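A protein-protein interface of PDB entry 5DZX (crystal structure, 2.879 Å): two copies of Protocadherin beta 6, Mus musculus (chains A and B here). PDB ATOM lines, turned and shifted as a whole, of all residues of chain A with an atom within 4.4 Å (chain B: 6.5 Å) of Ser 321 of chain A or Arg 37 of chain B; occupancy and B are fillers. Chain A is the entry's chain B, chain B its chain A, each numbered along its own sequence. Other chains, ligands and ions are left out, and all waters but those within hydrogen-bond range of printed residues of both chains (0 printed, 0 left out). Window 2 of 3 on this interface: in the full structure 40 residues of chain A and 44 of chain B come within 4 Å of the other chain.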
ATOM      1  N   THR A 319      -0.426 -19.786   7.214  1.00  0.00           N
ATOM      2  CA  THR A 319      -0.294 -18.455   7.791  1.00  0.00           C
ATOM      3  C   THR A 319       0.869 -17.694   7.158  1.00  0.00           C
ATOM      4  O   THR A 319       1.950 -18.251   6.959  1.00  0.00           O
ATOM      5  CB  THR A 319      -0.101 -18.526   9.317  1.00  0.00           C
ATOM      6  OG1 THR A 319       1.068 -19.300   9.616  1.00  0.00           O
ATOM      7  CG2 THR A 319      -1.307 -19.181   9.974  1.00  0.00           C
ATOM      8  N   ILE A 320       0.636 -16.424   6.840  1.00  0.00           N
ATOM      9  CA  ILE A 320       1.662 -15.590   6.222  1.00  0.00           C
ATOM     10  C   ILE A 320       2.416 -14.748   7.256  1.00  0.00           C
ATOM     11  O   ILE A 320       1.852 -13.852   7.886  1.00  0.00           O
ATOM     12  CB  ILE A 320       1.056 -14.674   5.126  1.00  0.00           C
ATOM     13  CG1 ILE A 320       2.116 -13.714   4.586  1.00  0.00           C
ATOM     14  CG2 ILE A 320      -0.181 -13.931   5.634  1.00  0.00           C
ATOM     15  CD1 ILE A 320       3.221 -14.411   3.833  1.00  0.00           C
ATOM     16  N   SER A 321       3.698 -15.054   7.432  1.00  0.00           N
ATOM     17  CA  SER A 321       4.533 -14.354   8.404  1.00  0.00           C
ATOM     18  C   SER A 321       5.044 -13.023   7.867  1.00  0.00           C
ATOM     19  O   SER A 321       4.899 -11.981   8.508  1.00  0.00           O
ATOM     20  CB  SER A 321       5.717 -15.231   8.816  1.00  0.00           C
ATOM     21  OG  SER A 321       5.279 -16.485   9.308  1.00  0.00           O
ATOM     22  N   SER A 322       5.655 -13.066   6.689  1.00  0.00           N
ATOM     23  CA  SER A 322       6.159 -11.859   6.053  1.00  0.00           C
ATOM     24  C   SER A 322       5.881 -11.889   4.558  1.00  0.00           C
ATOM     25  O   SER A 322       6.021 -12.924   3.910  1.00  0.00           O
ATOM     26  CB  SER A 322       7.658 -11.702   6.308  1.00  0.00           C
ATOM     27  OG  SER A 322       8.186 -10.609   5.577  1.00  0.00           O
ATOM     28  N   VAL A 338       7.162 -15.127   3.114  1.00  0.00           N
ATOM     29  CA  VAL A 338       7.546 -16.173   4.054  1.00  0.00           C
ATOM     30  C   VAL A 338       6.314 -16.694   4.783  1.00  0.00           C
ATOM     31  O   VAL A 338       5.654 -15.951   5.511  1.00  0.00           O
ATOM     32  CB  VAL A 338       8.571 -15.668   5.084  1.00  0.00           C
ATOM     33  CG1 VAL A 338       8.957 -16.786   6.042  1.00  0.00           C
ATOM     34  CG2 VAL A 338       9.799 -15.110   4.383  1.00  0.00           C
ATOM     35  N   PHE A 339       6.009 -17.973   4.591  1.00  0.00           N
ATOM     36  CA  PHE A 339       4.791 -18.547   5.144  1.00  0.00           C
ATOM     37  C   PHE A 339       5.067 -19.807   5.951  1.00  0.00           C
ATOM     38  O   PHE A 339       6.168 -20.360   5.915  1.00  0.00           O
ATOM     39  CB  PHE A 339       3.793 -18.859   4.026  1.00  0.00           C
ATOM     40  CG  PHE A 339       4.313 -19.832   3.000  1.00  0.00           C
ATOM     41  CD1 PHE A 339       4.092 -21.193   3.136  1.00  0.00           C
ATOM     42  CD2 PHE A 339       5.013 -19.385   1.893  1.00  0.00           C
ATOM     43  CE1 PHE A 339       4.565 -22.087   2.194  1.00  0.00           C
ATOM     44  CE2 PHE A 339       5.490 -20.275   0.949  1.00  0.00           C
ATOM     45  CZ  PHE A 339       5.264 -21.627   1.099  1.00  0.00           C
ATOM     46  N   SER A 340       4.053 -20.250   6.682  1.00  0.00           N
ATOM     47  CA  SER A 340       4.152 -21.467   7.473  1.00  0.00           C
ATOM     48  C   SER A 340       2.851 -22.255   7.413  1.00  0.00           C
ATOM     49  O   SER A 340       1.781 -21.695   7.169  1.00  0.00           O
ATOM     50  CB  SER A 340       4.504 -21.138   8.922  1.00  0.00           C
ATOM     51  OG  SER A 340       3.521 -20.296   9.493  1.00  0.00           O
ATOM     52  N   TYR A 371       8.201 -24.743   7.668  1.00  0.00           N
ATOM     53  CA  TYR A 371       8.467 -23.342   7.374  1.00  0.00           C
ATOM     54  C   TYR A 371       9.138 -23.193   6.015  1.00  0.00           C
ATOM     55  O   TYR A 371      10.260 -23.673   5.812  1.00  0.00           O
ATOM     56  CB  TYR A 371       9.348 -22.733   8.460  1.00  0.00           C
ATOM     57  CG  TYR A 371       8.591 -21.977   9.524  1.00  0.00           C
ATOM     58  CD1 TYR A 371       8.038 -22.640  10.611  1.00  0.00           C
ATOM     59  CD2 TYR A 371       8.439 -20.600   9.447  1.00  0.00           C
ATOM     60  CE1 TYR A 371       7.350 -21.952  11.589  1.00  0.00           C
ATOM     61  CE2 TYR A 371       7.752 -19.902  10.421  1.00  0.00           C
ATOM     62  CZ  TYR A 371       7.210 -20.582  11.490  1.00  0.00           C
ATOM     63  OH  TYR A 371       6.525 -19.892  12.463  1.00  0.00           O
ATOM     64  N   LEU B  31      16.659  -5.154  15.580  1.00  0.00           N
ATOM     65  CA  LEU B  31      15.302  -5.688  15.549  1.00  0.00           C
ATOM     66  C   LEU B  31      14.373  -4.768  14.770  1.00  0.00           C
ATOM     67  O   LEU B  31      13.523  -5.228  14.006  1.00  0.00           O
ATOM     68  CB  LEU B  31      14.771  -5.889  16.971  1.00  0.00           C
ATOM     69  CG  LEU B  31      15.372  -7.051  17.763  1.00  0.00           C
ATOM     70  CD1 LEU B  31      14.786  -7.100  19.163  1.00  0.00           C
ATOM     71  CD2 LEU B  31      15.126  -8.361  17.033  1.00  0.00           C
ATOM     72  N   ARG B  34      15.468  -4.978  10.858  1.00  0.00           N
ATOM     73  CA  ARG B  34      15.142  -6.226  10.170  1.00  0.00           C
ATOM     74  C   ARG B  34      13.655  -6.553  10.184  1.00  0.00           C
ATOM     75  O   ARG B  34      13.257  -7.628   9.734  1.00  0.00           O
ATOM     76  CB  ARG B  34      15.910  -7.401  10.780  1.00  0.00           C
ATOM     77  CG  ARG B  34      17.414  -7.284  10.688  1.00  0.00           C
ATOM     78  CD  ARG B  34      18.076  -8.567  11.153  1.00  0.00           C
ATOM     79  NE  ARG B  34      19.531  -8.471  11.112  1.00  0.00           N
ATOM     80  CZ  ARG B  34      20.352  -9.510  11.222  1.00  0.00           C
ATOM     81  NH1 ARG B  34      19.864 -10.733  11.374  1.00  0.00           N
ATOM     82  NH2 ARG B  34      21.664  -9.324  11.176  1.00  0.00           N
ATOM     83  N   ARG B  35      12.843  -5.630  10.696  1.00  0.00           N
ATOM     84  CA  ARG B  35      11.399  -5.828  10.789  1.00  0.00           C
ATOM     85  C   ARG B  35      11.086  -7.143  11.495  1.00  0.00           C
ATOM     86  O   ARG B  35      10.345  -7.981  10.978  1.00  0.00           O
ATOM     87  CB  ARG B  35      10.755  -5.800   9.399  1.00  0.00           C
ATOM     88  N   ALA B  36      11.660  -7.306  12.683  1.00  0.00           N
ATOM     89  CA  ALA B  36      11.516  -8.527  13.462  1.00  0.00           C
ATOM     90  C   ALA B  36      10.058  -8.792  13.778  1.00  0.00           C
ATOM     91  O   ALA B  36       9.344  -7.905  14.241  1.00  0.00           O
ATOM     92  CB  ALA B  36      12.322  -8.434  14.742  1.00  0.00           C
ATOM     93  N   ARG B  37       9.607 -10.012  13.510  1.00  0.00           N
ATOM     94  CA  ARG B  37       8.226 -10.365  13.817  1.00  0.00           C
ATOM     95  C   ARG B  37       8.147 -11.721  14.508  1.00  0.00           C
ATOM     96  O   ARG B  37       8.810 -12.668  14.099  1.00  0.00           O
ATOM     97  CB  ARG B  37       7.391 -10.364  12.533  1.00  0.00           C
ATOM     98  CG  ARG B  37       5.894 -10.465  12.754  1.00  0.00           C
ATOM     99  CD  ARG B  37       5.144 -10.261  11.448  1.00  0.00           C
ATOM    100  N   ILE B  38       7.329 -11.813  15.552  1.00  0.00           N
ATOM    101  CA  ILE B  38       7.203 -13.055  16.309  1.00  0.00           C
ATOM    102  C   ILE B  38       6.033 -13.885  15.789  1.00  0.00           C
ATOM    103  O   ILE B  38       4.952 -13.358  15.521  1.00  0.00           O
ATOM    104  CB  ILE B  38       7.021 -12.802  17.824  1.00  0.00           C
ATOM    105  CG1 ILE B  38       6.912 -14.136  18.569  1.00  0.00           C
ATOM    106  CG2 ILE B  38       5.808 -11.920  18.095  1.00  0.00           C
ATOM    107  CD1 ILE B  38       6.623 -14.000  20.038  1.00  0.00           C
ATOM    108  N   HIS B  39       6.255 -15.184  15.632  1.00  0.00           N
ATOM    109  CA  HIS B  39       5.228 -16.036  15.058  1.00  0.00           C
ATOM    110  C   HIS B  39       4.965 -17.292  15.889  1.00  0.00           C
ATOM    111  O   HIS B  39       5.880 -18.074  16.148  1.00  0.00           O
ATOM    112  CB  HIS B  39       5.635 -16.416  13.632  1.00  0.00           C
ATOM    113  CG  HIS B  39       4.496 -16.858  12.771  1.00  0.00           C
ATOM    114  ND1 HIS B  39       4.329 -18.166  12.373  1.00  0.00           N
ATOM    115  CD2 HIS B  39       3.470 -16.164  12.225  1.00  0.00           C
ATOM    116  CE1 HIS B  39       3.246 -18.261  11.623  1.00  0.00           C
ATOM    117  NE2 HIS B  39       2.706 -17.060  11.517  1.00  0.00           N
ATOM    118  N   LEU B  49       5.742  -8.992  19.885  1.00  0.00           N
ATOM    119  CA  LEU B  49       7.089  -8.455  20.035  1.00  0.00           C
ATOM    120  C   LEU B  49       7.160  -6.982  19.646  1.00  0.00           C
ATOM    121  O   LEU B  49       7.147  -6.642  18.463  1.00  0.00           O
ATOM    122  CB  LEU B  49       8.075  -9.265  19.190  1.00  0.00           C
ATOM    123  CG  LEU B  49       9.526  -8.783  19.108  1.00  0.00           C
ATOM    124  CD1 LEU B  49      10.187  -8.777  20.477  1.00  0.00           C
ATOM    125  CD2 LEU B  49      10.310  -9.650  18.136  1.00  0.00           C
ATOM    126  N   VAL B  51       9.079  -4.099  18.780  1.00  0.00           N
ATOM    127  CA  VAL B  51      10.420  -3.869  18.256  1.00  0.00           C
ATOM    128  C   VAL B  51      10.937  -2.475  18.594  1.00  0.00           C
ATOM    129  O   VAL B  51      12.127  -2.195  18.452  1.00  0.00           O
ATOM    130  CB  VAL B  51      10.465  -4.056  16.725  1.00  0.00           C
ATOM    131  CG1 VAL B  51      10.224  -5.511  16.358  1.00  0.00           C
ATOM    132  CG2 VAL B  51       9.445  -3.150  16.046  1.00  0.00           C
ATOM    133  N   GLN B  79       8.396 -19.223  17.011  1.00  0.00           N
ATOM    134  CA  GLN B  79       9.532 -18.921  16.156  1.00  0.00           C
ATOM    135  C   GLN B  79       9.498 -17.442  15.810  1.00  0.00           C
ATOM    136  O   GLN B  79       8.540 -16.957  15.203  1.00  0.00           O
ATOM    137  CB  GLN B  79       9.519 -19.766  14.879  1.00  0.00           C
ATOM    138  CG  GLN B  79       9.588 -21.265  15.108  1.00  0.00           C
ATOM    139  CD  GLN B  79       8.226 -21.880  15.369  1.00  0.00           C
ATOM    140  OE1 GLN B  79       7.213 -21.182  15.400  1.00  0.00           O
ATOM    141  NE2 GLN B  79       8.197 -23.195  15.556  1.00  0.00           N
ATOM    142  N   ILE B  80      10.529 -16.721  16.232  1.00  0.00           N
ATOM    143  CA  ILE B  80      10.662 -15.320  15.875  1.00  0.00           C
ATOM    144  C   ILE B  80      11.526 -15.216  14.622  1.00  0.00           C
ATOM    145  O   ILE B  80      12.514 -15.945  14.460  1.00  0.00           O
ATOM    146  CB  ILE B  80      11.248 -14.474  17.033  1.00  0.00           C
ATOM    147  CG1 ILE B  80      12.726 -14.787  17.265  1.00  0.00           C
ATOM    148  CG2 ILE B  80      10.461 -14.712  18.311  1.00  0.00           C
ATOM    149  CD1 ILE B  80      13.673 -13.731  16.723  1.00  0.00           C
ATOM    150  N   ILE B  81      11.124 -14.322  13.728  1.00  0.00           N
ATOM    151  CA  ILE B  81      11.757 -14.200  12.427  1.00  0.00           C
ATOM    152  C   ILE B  81      12.341 -12.811  12.180  1.00  0.00           C
ATOM    153  O   ILE B  81      11.794 -11.783  12.614  1.00  0.00           O
ATOM    154  CB  ILE B  81      10.762 -14.538  11.287  1.00  0.00           C
ATOM    155  CG1 ILE B  81       9.734 -13.419  11.105  1.00  0.00           C
ATOM    156  CG2 ILE B  81      10.061 -15.857  11.567  1.00  0.00           C
ATOM    157  CD1 ILE B  81       8.842 -13.599   9.899  1.00  0.00           C
ATOM    158  N   LEU B  82      13.479 -12.813  11.494  1.00  0.00           N
ATOM    159  CA  LEU B  82      14.145 -11.607  11.038  1.00  0.00           C
ATOM    160  C   LEU B  82      14.153 -11.649   9.516  1.00  0.00           C
ATOM    161  O   LEU B  82      14.545 -12.661   8.928  1.00  0.00           O
ATOM    162  CB  LEU B  82      15.567 -11.527  11.587  1.00  0.00           C
ATOM    163  CG  LEU B  82      15.727 -11.691  13.101  1.00  0.00           C
ATOM    164  CD1 LEU B  82      17.196 -11.677  13.485  1.00  0.00           C
ATOM    165  CD2 LEU B  82      14.967 -10.613  13.847  1.00  0.00           C
ATOM    166  N   GLU B  83      13.722 -10.561   8.882  1.00  0.00           N
ATOM    167  CA  GLU B  83      13.508 -10.556   7.438  1.00  0.00           C
ATOM    168  C   GLU B  83      14.806 -10.552   6.635  1.00  0.00           C
ATOM    169  O   GLU B  83      15.033 -11.437   5.810  1.00  0.00           O
ATOM    170  CB  GLU B  83      12.652  -9.353   7.030  1.00  0.00           C
ATOM    171  CG  GLU B  83      11.159  -9.540   7.270  1.00  0.00           C
ATOM    172  CD  GLU B  83      10.311  -8.525   6.524  1.00  0.00           C
ATOM    173  OE1 GLU B  83      10.855  -7.822   5.646  1.00  0.00           O
ATOM    174  OE2 GLU B  83       9.099  -8.429   6.816  1.00  0.00           O
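OE2 of Glu 83 of chain B is in hydrogen-bond range of OG of Ser 322 of chain A, at 2.7 Å.
A ring nitrogen (ND1) of His 39 of chain B lies within hydrogen-bond range of the side-chain hydroxyl of Tyr 371 of chain A (2.8 Å).
NE2 of His 39 of chain B sits close to OG1 of Thr 319 of chain A (3.4 Å).
The side-chain amide oxygen (OE1) of Gln 79 of chain B is in hydrogen-bond range of the side-chain hydroxyl (OH) of Tyr 371 of chain A (3.3 Å).
A ring nitrogen (NE2) of His 39 of chain B lies within hydrogen-bond range of the side-chain hydroxyl (OG) of Ser 321 of chain A.
N of Ser 321 of chain A lies within hydrogen-bond range of O of Val 338 of chain A.
O of Arg 34 of chain B sits at hydrogen-bond distance from N of Glu 83 of chain B.
O of Ser 322 of chain A sits at hydrogen-bond distance from N of Val 338 of chain A (2.6 Å).
N of Ile 81 of chain B is in hydrogen-bond range of O of Arg 37 of chain B, 2.9 Å away.
O of His 39 of chain B lies within hydrogen-bond range of N of Gln 79 of chain B, at 2.9 Å.
The side-chain hydroxyl (OG1) of Thr 319 of chain A is in hydrogen-bond range of the side-chain hydroxyl (OG) of Ser 340 of chain A (2.7 Å).
Ser 321 of chain A touches Arg 37 of chain B (O to CD, 3.4 Å).
Ser 321 of chain A touches Ile 81 of chain B.
His 39 of chain B touches Ser 340 of chain A.
Printed residues of chain B within 4 Å of Ser 321 of chain A: Arg 37, His 39 and Ile 81.
Arg 37 of chain B touches one residue of chain A.
Printed residues of chain A within 4 Å of His 39 of chain B: Thr 319, Ser 321, Ser 340 and Tyr 371.
Printed residues of chain A within 4 Å of Glu 83 of chain B: Ser 322 (2.7 Å).
Of the printed residues of chain B, Ser 322 of chain A touches Glu 83 (2.7 Å).
Of the printed residues of chain A, Gln 79 of chain B touches Tyr 371.
Printed residues of chain B within 4 Å of Thr 319 of chain A: His 39 (3.1 Å).
Leu 31 of chain B touches none of the printed residues of chain A.
Val 338 of chain A touches none of the printed residues of chain B.
The nearest printed residue of chain A that does not touch Arg 37 of chain B is Ser 322 of chain A (5.5 Å).
The nearest printed residue of chain B that does not touch Tyr 371 of chain A is Ile 81 of chain B (4.8 Å).
Of the 8 printed residues of chain A, 5 touch a printed residue of chain B.
Along chain A the printed residues that touch a printed residue of chain B span positions 319 to 371.
Among the printed residues, no Asp or Glu carboxylate lies within 4 Å of a Lys or Arg side-chain nitrogen of the other chain.
No position is printed for both chains.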
